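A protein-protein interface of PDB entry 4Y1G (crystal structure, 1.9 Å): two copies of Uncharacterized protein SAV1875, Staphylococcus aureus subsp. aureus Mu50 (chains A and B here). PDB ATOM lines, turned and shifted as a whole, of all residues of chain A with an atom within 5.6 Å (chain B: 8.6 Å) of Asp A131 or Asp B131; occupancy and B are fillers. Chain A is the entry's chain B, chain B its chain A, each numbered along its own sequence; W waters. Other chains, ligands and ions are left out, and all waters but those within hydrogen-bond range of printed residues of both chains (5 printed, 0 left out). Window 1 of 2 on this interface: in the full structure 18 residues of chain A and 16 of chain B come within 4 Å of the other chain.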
ATOM      1  N   ARG A  80       2.390  25.415   8.722  1.00  0.00           N
ATOM      2  CA  ARG A  80       2.789  25.280  10.125  1.00  0.00           C
ATOM      3  C   ARG A  80       4.001  26.138  10.485  1.00  0.00           C
ATOM      4  O   ARG A  80       4.355  26.260  11.664  1.00  0.00           O
ATOM      5  CB  ARG A  80       3.102  23.802  10.443  1.00  0.00           C
ATOM      6  CG  ARG A  80       1.850  22.936  10.370  1.00  0.00           C
ATOM      7  CD  ARG A  80       2.146  21.497  10.749  1.00  0.00           C
ATOM      8  NE  ARG A  80       2.005  21.282  12.186  1.00  0.00           N
ATOM      9  CZ  ARG A  80       2.397  20.168  12.796  1.00  0.00           C
ATOM     10  NH1 ARG A  80       3.115  19.276  12.119  1.00  0.00           N
ATOM     11  NH2 ARG A  80       2.121  19.971  14.083  1.00  0.00           N
ATOM     12  N   GLN A 109      -1.730  17.098   9.326  1.00  0.00           N
ATOM     13  CA  GLN A 109      -0.710  17.759  10.165  1.00  0.00           C
ATOM     14  C   GLN A 109      -1.217  19.060  10.769  1.00  0.00           C
ATOM     15  O   GLN A 109      -0.860  19.434  11.894  1.00  0.00           O
ATOM     16  CB  GLN A 109       0.520  18.096   9.319  1.00  0.00           C
ATOM     17  CG  GLN A 109       1.416  16.901   9.126  1.00  0.00           C
ATOM     18  CD  GLN A 109       2.675  17.270   8.387  1.00  0.00           C
ATOM     19  OE1 GLN A 109       2.628  17.868   7.302  1.00  0.00           O
ATOM     20  NE2 GLN A 109       3.813  16.926   8.973  1.00  0.00           N
ATOM     21  N   ILE A 112      -3.217  18.801  13.913  1.00  0.00           N
ATOM     22  CA  ILE A 112      -2.457  18.578  15.137  1.00  0.00           C
ATOM     23  C   ILE A 112      -2.340  19.899  15.881  1.00  0.00           C
ATOM     24  O   ILE A 112      -2.417  19.947  17.114  1.00  0.00           O
ATOM     25  CB  ILE A 112      -1.042  18.046  14.828  1.00  0.00           C
ATOM     26  CG1 ILE A 112      -1.137  16.625  14.267  1.00  0.00           C
ATOM     27  CG2 ILE A 112      -0.175  18.066  16.078  1.00  0.00           C
ATOM     28  CD1 ILE A 112       0.189  16.060  13.778  1.00  0.00           C
ATOM     29  N   ASN A 127       3.658   8.766   6.504  1.00  0.00           N
ATOM     30  CA  ASN A 127       4.744   9.622   7.019  1.00  0.00           C
ATOM     31  C   ASN A 127       4.341  10.444   8.269  1.00  0.00           C
ATOM     32  O   ASN A 127       5.204  10.975   8.972  1.00  0.00           O
ATOM     33  CB  ASN A 127       5.238  10.601   5.924  1.00  0.00           C
ATOM     34  CG  ASN A 127       5.563   9.907   4.608  1.00  0.00           C
ATOM     35  OD1 ASN A 127       6.660  10.080   4.045  1.00  0.00           O
ATOM     36  ND2 ASN A 127       4.596   9.186   4.070  1.00  0.00           N
ATOM     37  N   VAL A 128       3.048  10.726   8.413  1.00  0.00           N
ATOM     38  CA  VAL A 128       2.598  11.592   9.501  1.00  0.00           C
ATOM     39  C   VAL A 128       1.770  10.860  10.570  1.00  0.00           C
ATOM     40  O   VAL A 128       1.302  11.471  11.533  1.00  0.00           O
ATOM     41  CB  VAL A 128       1.804  12.804   8.961  1.00  0.00           C
ATOM     42  CG1 VAL A 128       2.557  13.467   7.805  1.00  0.00           C
ATOM     43  CG2 VAL A 128       0.415  12.389   8.530  1.00  0.00           C
ATOM     44  N   ARG A 129       1.582   9.552  10.413  1.00  0.00           N
ATOM     45  CA  ARG A 129       0.710   8.823  11.325  1.00  0.00           C
ATOM     46  C   ARG A 129       1.228   8.854  12.751  1.00  0.00           C
ATOM     47  O   ARG A 129       0.445   8.754  13.698  1.00  0.00           O
ATOM     48  CB  ARG A 129       0.556   7.362  10.889  1.00  0.00           C
ATOM     49  CG  ARG A 129      -0.372   7.265   9.697  1.00  0.00           C
ATOM     50  CD  ARG A 129      -0.607   5.830   9.255  1.00  0.00           C
ATOM     51  NE  ARG A 129      -1.180   5.895   7.914  1.00  0.00           N
ATOM     52  CZ  ARG A 129      -1.161   4.905   7.039  1.00  0.00           C
ATOM     53  NH1 ARG A 129      -0.723   3.704   7.395  1.00  0.00           N
ATOM     54  NH2 ARG A 129      -1.631   5.120   5.820  1.00  0.00           N
ATOM     55  N   LYS A 130       2.544   8.832  12.918  1.00  0.00           N
ATOM     56  CA  LYS A 130       3.057   8.755  14.276  1.00  0.00           C
ATOM     57  C   LYS A 130       2.775  10.076  14.977  1.00  0.00           C
ATOM     58  O   LYS A 130       2.540  10.111  16.190  1.00  0.00           O
ATOM     59  CB  LYS A 130       4.557   8.433  14.299  1.00  0.00           C
ATOM     60  CG  LYS A 130       5.138   8.493  15.709  1.00  0.00           C
ATOM     61  CD  LYS A 130       4.679   7.327  16.578  1.00  0.00           C
ATOM     62  CE  LYS A 130       5.625   7.175  17.760  1.00  0.00           C
ATOM     63  NZ  LYS A 130       5.010   6.395  18.867  1.00  0.00           N
ATOM     64  N   ASP A 131       2.837  11.173  14.232  1.00  0.00           N
ATOM     65  CA  ASP A 131       2.546  12.466  14.829  1.00  0.00           C
ATOM     66  C   ASP A 131       1.075  12.597  15.216  1.00  0.00           C
ATOM     67  O   ASP A 131       0.732  13.183  16.261  1.00  0.00           O
ATOM     68  CB  ASP A 131       3.004  13.595  13.905  1.00  0.00           C
ATOM     69  CG  ASP A 131       4.530  13.627  13.745  1.00  0.00           C
ATOM     70  OD1 ASP A 131       5.242  13.171  14.679  1.00  0.00           O
ATOM     71  OD2 ASP A 131       5.019  13.967  12.644  1.00  0.00           O
ATOM     72  N   LEU A 132       0.206  11.988  14.417  1.00  0.00           N
ATOM     73  CA  LEU A 132      -1.212  11.980  14.751  1.00  0.00           C
ATOM     74  C   LEU A 132      -1.454  11.138  16.007  1.00  0.00           C
ATOM     75  O   LEU A 132      -2.256  11.516  16.866  1.00  0.00           O
ATOM     76  CB  LEU A 132      -2.040  11.433  13.583  1.00  0.00           C
ATOM     77  CG  LEU A 132      -2.070  12.333  12.337  1.00  0.00           C
ATOM     78  CD1 LEU A 132      -2.768  11.576  11.212  1.00  0.00           C
ATOM     79  CD2 LEU A 132      -2.809  13.642  12.650  1.00  0.00           C
ATOM     80  N   SER A 133      -0.760  10.009  16.103  1.00  0.00           N
ATOM     81  CA  SER A 133      -0.827   9.147  17.297  1.00  0.00           C
ATOM     82  C   SER A 133      -0.381   9.877  18.583  1.00  0.00           C
ATOM     83  O   SER A 133      -1.076   9.844  19.602  1.00  0.00           O
ATOM     84  CB  SER A 133       0.025   7.875  17.078  1.00  0.00           C
ATOM     85  OG  SER A 133      -0.075   7.014  18.207  1.00  0.00           O
ATOM     86  N   ASN A 134       0.731  10.608  18.499  1.00  0.00           N
ATOM     87  CA  ASN A 134       1.253  11.376  19.636  1.00  0.00           C
ATOM     88  C   ASN A 134       0.302  12.509  20.024  1.00  0.00           C
ATOM     89  O   ASN A 134       0.303  12.968  21.167  1.00  0.00           O
ATOM     90  CB  ASN A 134       2.639  11.949  19.298  1.00  0.00           C
ATOM     91  CG  ASN A 134       3.740  10.921  19.481  1.00  0.00           C
ATOM     92  OD1 ASN A 134       3.492   9.846  20.016  1.00  0.00           O
ATOM     93  ND2 ASN A 134       4.890  11.164  18.890  1.00  0.00           N
ATOM     94  N   ALA A 135      -0.493  12.966  19.065  1.00  0.00           N
ATOM     95  CA  ALA A 135      -1.483  14.022  19.315  1.00  0.00           C
ATOM     96  C   ALA A 135      -2.726  13.466  20.012  1.00  0.00           C
ATOM     97  O   ALA A 135      -3.647  14.219  20.352  1.00  0.00           O
ATOM     98  CB  ALA A 135      -1.886  14.689  18.007  1.00  0.00           C
ATOM     99  N   GLY A 136      -2.793  12.145  20.108  1.00  0.00           N
ATOM    100  CA  GLY A 136      -3.862  11.468  20.865  1.00  0.00           C
ATOM    101  C   GLY A 136      -4.952  10.851  20.001  1.00  0.00           C
ATOM    102  O   GLY A 136      -5.968  10.392  20.517  1.00  0.00           O
ATOM    103  N   ASP B  77      11.042  13.796   6.324  1.00  0.00           N
ATOM    104  CA  ASP B  77       9.702  13.325   5.953  1.00  0.00           C
ATOM    105  C   ASP B  77       9.739  12.111   5.017  1.00  0.00           C
ATOM    106  O   ASP B  77       9.024  11.117   5.219  1.00  0.00           O
ATOM    107  CB  ASP B  77       8.879  14.444   5.329  1.00  0.00           C
ATOM    108  CG  ASP B  77       7.413  14.062   5.176  1.00  0.00           C
ATOM    109  OD1 ASP B  77       6.646  14.212   6.150  1.00  0.00           O
ATOM    110  OD2 ASP B  77       7.049  13.531   4.113  1.00  0.00           O
ATOM    111  N   ARG B  80      10.730   8.950   6.913  1.00  0.00           N
ATOM    112  CA  ARG B  80       9.622   8.422   7.711  1.00  0.00           C
ATOM    113  C   ARG B  80       8.551   7.742   6.864  1.00  0.00           C
ATOM    114  O   ARG B  80       7.583   7.196   7.399  1.00  0.00           O
ATOM    115  CB  ARG B  80       8.993   9.549   8.542  1.00  0.00           C
ATOM    116  CG  ARG B  80       9.951  10.122   9.577  1.00  0.00           C
ATOM    117  CD  ARG B  80       9.302  11.298  10.301  1.00  0.00           C
ATOM    118  NE  ARG B  80       8.575  10.860  11.497  1.00  0.00           N
ATOM    119  CZ  ARG B  80       7.726  11.632  12.169  1.00  0.00           C
ATOM    120  NH1 ARG B  80       7.319  12.783  11.642  1.00  0.00           N
ATOM    121  NH2 ARG B  80       7.213  11.209  13.319  1.00  0.00           N
ATOM    122  N   HIS B 106      14.196  20.317  10.275  1.00  0.00           N
ATOM    123  CA  HIS B 106      13.259  19.186  10.363  1.00  0.00           C
ATOM    124  C   HIS B 106      13.854  17.877  10.870  1.00  0.00           C
ATOM    125  O   HIS B 106      13.121  16.916  11.112  1.00  0.00           O
ATOM    126  CB  HIS B 106      12.616  18.922   8.990  1.00  0.00           C
ATOM    127  CG  HIS B 106      11.556  19.929   8.617  1.00  0.00           C
ATOM    128  ND1 HIS B 106      11.850  21.136   8.073  1.00  0.00           N
ATOM    129  CD2 HIS B 106      10.166  19.864   8.699  1.00  0.00           C
ATOM    130  CE1 HIS B 106      10.700  21.786   7.793  1.00  0.00           C
ATOM    131  NE2 HIS B 106       9.675  21.001   8.162  1.00  0.00           N
ATOM    132  N   PRO B 108      14.935  16.658  13.635  1.00  0.00           N
ATOM    133  CA  PRO B 108      14.378  16.054  14.849  1.00  0.00           C
ATOM    134  C   PRO B 108      13.080  15.268  14.662  1.00  0.00           C
ATOM    135  O   PRO B 108      12.755  14.416  15.487  1.00  0.00           O
ATOM    136  CB  PRO B 108      14.157  17.269  15.748  1.00  0.00           C
ATOM    137  CG  PRO B 108      15.283  18.166  15.370  1.00  0.00           C
ATOM    138  CD  PRO B 108      15.254  18.081  13.860  1.00  0.00           C
ATOM    139  N   GLN B 109      12.440  15.397  13.504  1.00  0.00           N
ATOM    140  CA  GLN B 109      11.332  14.511  13.184  1.00  0.00           C
ATOM    141  C   GLN B 109      11.687  13.028  13.325  1.00  0.00           C
ATOM    142  O   GLN B 109      10.819  12.221  13.605  1.00  0.00           O
ATOM    143  CB  GLN B 109      10.824  14.776  11.765  1.00  0.00           C
ATOM    144  CG  GLN B 109       9.849  15.934  11.692  1.00  0.00           C
ATOM    145  CD  GLN B 109       9.319  16.155  10.291  1.00  0.00           C
ATOM    146  OE1 GLN B 109      10.084  16.231   9.322  1.00  0.00           O
ATOM    147  NE2 GLN B 109       8.002  16.284  10.177  1.00  0.00           N
ATOM    148  N   ILE B 110      12.856  12.635  12.834  1.00  0.00           N
ATOM    149  CA  ILE B 110      13.225  11.223  12.898  1.00  0.00           C
ATOM    150  C   ILE B 110      13.320  10.764  14.365  1.00  0.00           C
ATOM    151  O   ILE B 110      13.075   9.596  14.681  1.00  0.00           O
ATOM    152  CB  ILE B 110      14.578  10.959  12.182  1.00  0.00           C
ATOM    153  CG1 ILE B 110      14.398  11.103  10.667  1.00  0.00           C
ATOM    154  CG2 ILE B 110      15.076   9.546  12.488  1.00  0.00           C
ATOM    155  CD1 ILE B 110      13.526  10.019  10.073  1.00  0.00           C
ATOM    156  N   LEU B 111      13.805  11.642  15.232  1.00  0.00           N
ATOM    157  CA  LEU B 111      13.957  11.277  16.644  1.00  0.00           C
ATOM    158  C   LEU B 111      12.612  10.955  17.263  1.00  0.00           C
ATOM    159  O   LEU B 111      12.535  10.198  18.226  1.00  0.00           O
ATOM    160  CB  LEU B 111      14.643  12.398  17.431  1.00  0.00           C
ATOM    161  CG  LEU B 111      16.054  12.698  16.897  1.00  0.00           C
ATOM    162  CD1 LEU B 111      16.689  13.820  17.699  1.00  0.00           C
ATOM    163  CD2 LEU B 111      16.920  11.436  16.908  1.00  0.00           C
ATOM    164  N   ILE B 112      11.555  11.612  16.791  1.00  0.00           N
ATOM    165  CA  ILE B 112      10.235  11.261  17.287  1.00  0.00           C
ATOM    166  C   ILE B 112       9.974   9.758  17.138  1.00  0.00           C
ATOM    167  O   ILE B 112       9.328   9.127  17.985  1.00  0.00           O
ATOM    168  CB  ILE B 112       9.136  12.062  16.567  1.00  0.00           C
ATOM    169  CG1 ILE B 112       9.279  13.570  16.885  1.00  0.00           C
ATOM    170  CG2 ILE B 112       7.754  11.530  16.942  1.00  0.00           C
ATOM    171  CD1 ILE B 112       8.409  14.453  16.001  1.00  0.00           C
ATOM    172  N   ASP B 113      10.461   9.177  16.049  1.00  0.00           N
ATOM    173  CA  ASP B 113      10.169   7.776  15.769  1.00  0.00           C
ATOM    174  C   ASP B 113      10.919   6.795  16.661  1.00  0.00           C
ATOM    175  O   ASP B 113      10.519   5.629  16.752  1.00  0.00           O
ATOM    176  CB  ASP B 113      10.435   7.459  14.303  1.00  0.00           C
ATOM    177  CG  ASP B 113       9.472   8.181  13.385  1.00  0.00           C
ATOM    178  OD1 ASP B 113       8.362   8.542  13.849  1.00  0.00           O
ATOM    179  OD2 ASP B 113       9.829   8.408  12.212  1.00  0.00           O
ATOM    180  N   LEU B 117      12.122  10.334  23.511  1.00  0.00           N
ATOM    181  CA  LEU B 117      12.262  11.787  23.719  1.00  0.00           C
ATOM    182  C   LEU B 117      11.684  12.277  25.042  1.00  0.00           C
ATOM    183  O   LEU B 117      11.793  13.463  25.353  1.00  0.00           O
ATOM    184  CB  LEU B 117      11.623  12.588  22.568  1.00  0.00           C
ATOM    185  CG  LEU B 117      12.276  12.405  21.201  1.00  0.00           C
ATOM    186  CD1 LEU B 117      11.704  13.409  20.192  1.00  0.00           C
ATOM    187  CD2 LEU B 117      13.779  12.561  21.335  1.00  0.00           C
ATOM    188  N   ALA B 124      14.004  22.752  17.420  1.00  0.00           N
ATOM    189  CA  ALA B 124      13.878  22.372  16.013  1.00  0.00           C
ATOM    190  C   ALA B 124      13.281  23.562  15.263  1.00  0.00           C
ATOM    191  O   ALA B 124      12.972  24.581  15.867  1.00  0.00           O
ATOM    192  CB  ALA B 124      12.973  21.137  15.875  1.00  0.00           C
ATOM    193  N   VAL B 125      13.119  23.441  13.949  1.00  0.00           N
ATOM    194  CA  VAL B 125      12.412  24.496  13.231  1.00  0.00           C
ATOM    195  C   VAL B 125      10.975  24.621  13.760  1.00  0.00           C
ATOM    196  O   VAL B 125      10.393  23.643  14.235  1.00  0.00           O
ATOM    197  CB  VAL B 125      12.447  24.245  11.717  1.00  0.00           C
ATOM    198  CG1 VAL B 125      11.566  23.049  11.348  1.00  0.00           C
ATOM    199  CG2 VAL B 125      12.099  25.509  10.939  1.00  0.00           C
ATOM    200  N   LEU B 126      10.431  25.841  13.747  1.00  0.00           N
ATOM    201  CA  LEU B 126       9.097  26.078  14.273  1.00  0.00           C
ATOM    202  C   LEU B 126       8.064  25.059  13.759  1.00  0.00           C
ATOM    203  O   LEU B 126       7.201  24.597  14.530  1.00  0.00           O
ATOM    204  CB  LEU B 126       8.636  27.516  13.952  1.00  0.00           C
ATOM    205  CG  LEU B 126       7.163  27.793  14.265  1.00  0.00           C
ATOM    206  CD1 LEU B 126       6.894  27.746  15.770  1.00  0.00           C
ATOM    207  CD2 LEU B 126       6.724  29.130  13.671  1.00  0.00           C
ATOM    208  N   ASN B 127       8.167  24.693  12.476  1.00  0.00           N
ATOM    209  CA  ASN B 127       7.166  23.847  11.815  1.00  0.00           C
ATOM    210  C   ASN B 127       6.938  22.516  12.570  1.00  0.00           C
ATOM    211  O   ASN B 127       5.885  21.874  12.432  1.00  0.00           O
ATOM    212  CB  ASN B 127       7.568  23.520  10.357  1.00  0.00           C
ATOM    213  CG  ASN B 127       7.924  24.755   9.542  1.00  0.00           C
ATOM    214  OD1 ASN B 127       7.495  24.920   8.373  1.00  0.00           O
ATOM    215  ND2 ASN B 127       8.689  25.636  10.149  1.00  0.00           N
ATOM    216  N   VAL B 128       7.946  22.105  13.333  1.00  0.00           N
ATOM    217  CA  VAL B 128       8.039  20.752  13.846  1.00  0.00           C
ATOM    218  C   VAL B 128       7.976  20.711  15.387  1.00  0.00           C
ATOM    219  O   VAL B 128       7.823  19.647  15.985  1.00  0.00           O
ATOM    220  CB  VAL B 128       9.326  20.118  13.254  1.00  0.00           C
ATOM    221  CG1 VAL B 128      10.292  19.600  14.280  1.00  0.00           C
ATOM    222  CG2 VAL B 128       9.008  19.155  12.127  1.00  0.00           C
ATOM    223  N   ARG B 129       7.925  21.882  16.021  1.00  0.00           N
ATOM    224  CA  ARG B 129       8.022  21.947  17.478  1.00  0.00           C
ATOM    225  C   ARG B 129       6.823  21.355  18.220  1.00  0.00           C
ATOM    226  O   ARG B 129       6.987  20.754  19.280  1.00  0.00           O
ATOM    227  CB  ARG B 129       8.266  23.375  17.949  1.00  0.00           C
ATOM    228  CG  ARG B 129       9.691  23.834  17.702  1.00  0.00           C
ATOM    229  CD  ARG B 129       9.904  25.213  18.323  1.00  0.00           C
ATOM    230  NE  ARG B 129      10.963  25.849  17.582  1.00  0.00           N
ATOM    231  CZ  ARG B 129      11.001  27.120  17.224  1.00  0.00           C
ATOM    232  NH1 ARG B 129      10.225  28.017  17.818  1.00  0.00           N
ATOM    233  NH2 ARG B 129      11.983  27.511  16.431  1.00  0.00           N
ATOM    234  N   LYS B 130       5.628  21.508  17.666  1.00  0.00           N
ATOM    235  CA  LYS B 130       4.432  20.928  18.280  1.00  0.00           C
ATOM    236  C   LYS B 130       4.562  19.407  18.321  1.00  0.00           C
ATOM    237  O   LYS B 130       4.198  18.757  19.310  1.00  0.00           O
ATOM    238  CB  LYS B 130       3.165  21.321  17.494  1.00  0.00           C
ATOM    239  CG  LYS B 130       1.870  20.799  18.115  1.00  0.00           C
ATOM    240  CD  LYS B 130       1.764  21.206  19.570  1.00  0.00           C
ATOM    241  CE  LYS B 130       0.927  22.467  19.703  1.00  0.00           C
ATOM    242  NZ  LYS B 130       0.048  22.392  20.901  1.00  0.00           N
ATOM    243  N   ASP B 131       5.044  18.834  17.227  1.00  0.00           N
ATOM    244  CA  ASP B 131       5.174  17.377  17.139  1.00  0.00           C
ATOM    245  C   ASP B 131       6.222  16.856  18.133  1.00  0.00           C
ATOM    246  O   ASP B 131       6.055  15.791  18.728  1.00  0.00           O
ATOM    247  CB  ASP B 131       5.506  16.970  15.700  1.00  0.00           C
ATOM    248  CG  ASP B 131       4.357  17.275  14.737  1.00  0.00           C
ATOM    249  OD1 ASP B 131       3.187  17.301  15.198  1.00  0.00           O
ATOM    250  OD2 ASP B 131       4.619  17.579  13.547  1.00  0.00           O
ATOM    251  N   LEU B 132       7.282  17.629  18.347  1.00  0.00           N
ATOM    252  CA  LEU B 132       8.306  17.256  19.323  1.00  0.00           C
ATOM    253  C   LEU B 132       7.717  17.301  20.727  1.00  0.00           C
ATOM    254  O   LEU B 132       7.923  16.390  21.526  1.00  0.00           O
ATOM    255  CB  LEU B 132       9.476  18.236  19.247  1.00  0.00           C
ATOM    256  CG  LEU B 132      10.910  17.822  18.998  1.00  0.00           C
ATOM    257  CD1 LEU B 132      11.006  16.499  18.244  1.00  0.00           C
ATOM    258  CD2 LEU B 132      11.624  18.960  18.263  1.00  0.00           C
ATOM    259  N   SER B 133       6.929  18.332  21.007  1.00  0.00           N
ATOM    260  CA  SER B 133       6.270  18.424  22.283  1.00  0.00           C
ATOM    261  C   SER B 133       5.338  17.245  22.516  1.00  0.00           C
ATOM    262  O   SER B 133       5.253  16.732  23.636  1.00  0.00           O
ATOM    263  CB  SER B 133       5.487  19.731  22.394  1.00  0.00           C
ATOM    264  OG  SER B 133       5.212  19.978  23.741  1.00  0.00           O
ATOM    265  N   ASN B 134       4.509  16.933  21.517  1.00  0.00           N
ATOM    266  CA  ASN B 134       3.595  15.795  21.642  1.00  0.00           C
ATOM    267  C   ASN B 134       4.333  14.454  21.839  1.00  0.00           C
ATOM    268  O   ASN B 134       3.784  13.511  22.389  1.00  0.00           O
ATOM    269  CB  ASN B 134       2.649  15.709  20.430  1.00  0.00           C
ATOM    270  CG  ASN B 134       1.555  16.768  20.460  1.00  0.00           C
ATOM    271  OD1 ASN B 134       1.262  17.334  21.500  1.00  0.00           O
ATOM    272  ND2 ASN B 134       0.878  16.956  19.340  1.00  0.00           N
ATOM    273  N   ALA B 135       5.581  14.379  21.405  1.00  0.00           N
ATOM    274  CA  ALA B 135       6.382  13.166  21.609  1.00  0.00           C
ATOM    275  C   ALA B 135       6.987  13.115  23.017  1.00  0.00           C
ATOM    276  O   ALA B 135       7.792  12.221  23.323  1.00  0.00           O
ATOM    277  CB  ALA B 135       7.481  13.085  20.561  1.00  0.00           C
ATOM    278  N   GLY B 136       6.810  14.207  23.750  1.00  0.00           N
ATOM    279  CA  GLY B 136       7.181  14.267  25.158  1.00  0.00           C
ATOM    280  C   GLY B 136       8.482  15.003  25.440  1.00  0.00           C
ATOM    281  O   GLY B 136       8.897  15.096  26.597  1.00  0.00           O
ATOM    282  N   ALA B 137       9.045  15.658  24.429  1.00  0.00           N
ATOM    283  CA  ALA B 137      10.230  16.511  24.661  1.00  0.00           C
ATOM    284  C   ALA B 137       9.858  17.799  25.381  1.00  0.00           C
ATOM    285  O   ALA B 137       8.747  18.305  25.219  1.00  0.00           O
ATOM    286  CB  ALA B 137      10.930  16.842  23.340  1.00  0.00           C
ATOM    287  N   VAL B 139      10.450  21.251  24.745  1.00  0.00           N
ATOM    288  CA  VAL B 139      10.899  21.984  23.566  1.00  0.00           C
ATOM    289  C   VAL B 139      11.213  23.425  23.938  1.00  0.00           C
ATOM    290  O   VAL B 139      10.404  24.112  24.575  1.00  0.00           O
ATOM    291  CB  VAL B 139       9.866  21.921  22.414  1.00  0.00           C
ATOM    292  CG1 VAL B 139      10.420  22.606  21.175  1.00  0.00           C
ATOM    293  CG2 VAL B 139       9.522  20.470  22.096  1.00  0.00           C
HETATM  294  O   HOH W   1       2.140  15.418  17.141  1.00  0.00           O
HETATM  295  O   HOH W   2       4.736  13.697  17.436  1.00  0.00           O
HETATM  296  O   HOH W   3       7.330   9.457  19.822  1.00  0.00           O
HETATM  297  O   HOH W   4       7.002  13.239   8.592  1.00  0.00           O
HETATM  298  O   HOH W   5      -1.691  18.462  19.267  1.00  0.00           O
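OD2 of Asp B113 lies within salt-bridge range of NE of Arg B80 (2.8 Å).
The backbone carbonyl oxygen of Gln A109 sits at hydrogen-bond distance from the guanidinium group of Arg A80 (3.4 Å).
The guanidinium group (NE) of Arg B80 is in hydrogen-bond range of the backbone carbonyl oxygen (O) of Gln B109, 3.4 Å away.
Among the printed residues, merely in contact across the chains: Arg A80 with Asn B127 (3.7 Å), Arg A80 with Lys B130 (3.8 Å), Ile A112 with Lys B130 (3.98 Å), Ile A112 with Asp B131 (3.5 Å), Ile A112 with Asn B134 (3.6 Å), Asn A127 with Arg B80 (3.8 Å), Lys A130 with Arg B80 (3.96 Å), Lys A130 with Asp B113 (3.7 Å), Asp A131 with Ile B112 (3.7 Å), Asp A131 with Asp B131 (3.7 Å), Asn A134 with Ile B112 (3.5 Å), Asn A134 with Asn B134 (3.6 Å), Asn A134 with Ala B135 (3.6 Å) and Ala A135 with Asn B134 (3.8 Å).
Of the printed residues of chain B, Asn A127 touches Asp B77 (2.8 Å) and Arg B80 (3.8 Å).
Of the printed residues of chain B, Lys A130 touches Arg B80 and Asp B113.
Of chain B, only Arg B80, Ile B112 and Asp B131 come within 4 Å of Asp A131.
Printed residues of chain A within 4 Å of Arg B80: Asn A127 (3.8 Å), Lys A130 (3.96 Å) and Asp A131 (2.8 Å).
Printed residues of chain A within 4 Å of Lys B130: Arg A80 and Ile A112.
Printed residues of chain A within 4 Å of Ala B135: Asn A134.
The nearest residue of chain A that does not touch Asp B131 is Gln A109 (4.7 Å).
The nearest printed residue of chain B that does not touch Asn A134 is Asp B131 (4.8 Å).
Printed residues of chain B that touch a printed residue of chain A: Asp B77, Arg B80, Ile B112, Asp B113, Asn B127, Lys B130, Asp B131, Asn B134 and Ala B135.
Hydrophobic or aromatic side chains of chain B that line the printed part of chain A: Ile B112 and Ala B135.
Of the 13 printed residues of chain A, 7 touch a printed residue of chain B.
Along chain A the printed residues that touch a printed residue of chain B span positions 80 to 135.
Among the printed residues, 17 pairs touch across the chains.
The guanidinium group of Arg B80 lies within salt-bridge range of the side-chain carboxylate of Asp A131, at 2.8 Å.
O of Asp B77 lies close to OD1 of Asn A127.
The guanidinium group of Arg A80 lies within salt-bridge range of the side-chain carboxylate of Asp B131.
Arg A80 touches Asn B127, and with the chains exchanged Asn A127 touches Arg B80.
Arg A80 touches Asp B131, and with the chains exchanged Asp A131 touches Arg B80.
Ile A112 touches Lys B130, but with the chains exchanged Lys A130 does not touch Ile B112 (4.2 Å).
Asn A134 touches Ala B135, and with the chains exchanged Ala A135 touches Asn B134.
Positions printed for both chains: 80, 109, 112, 127, 128, 129, 130, 131, 132, 133, 134, 135 and 136.
Of the 17 pairs that touch across the chains among the printed residues, 14 have their exchanged pair printed and touching as well.
Water W4 lies within hydrogen-bond range of OD1 of Asp B77 (2.7 Å), O of Asn A127 (2.9 Å) and NH1 of Arg B80 (3.1 Å).
Water W5 bridges the backbone carbonyl oxygen of Ile A112 (2.7 Å) and the side-chain amide nitrogen of Asn B134 (3.0 Å).
Water W3 bridges O of Ile B112 and ND2 of Asn A134.
Water W1 lies within hydrogen-bond range of the backbone carbonyl oxygen of Asp A131 (2.8 Å), the side-chain carboxylate of Asp B131 (2.9 Å) and the side-chain amide nitrogen of Asn B134 (3.0 Å).
Water W2 lies within hydrogen-bond range of the backbone carbonyl oxygen (O) of Asp B131 (2.8 Å), the side-chain carboxylate (OD1) of Asp A131 (2.9 Å) and the side-chain amide nitrogen (ND2) of Asn A134 (2.9 Å).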
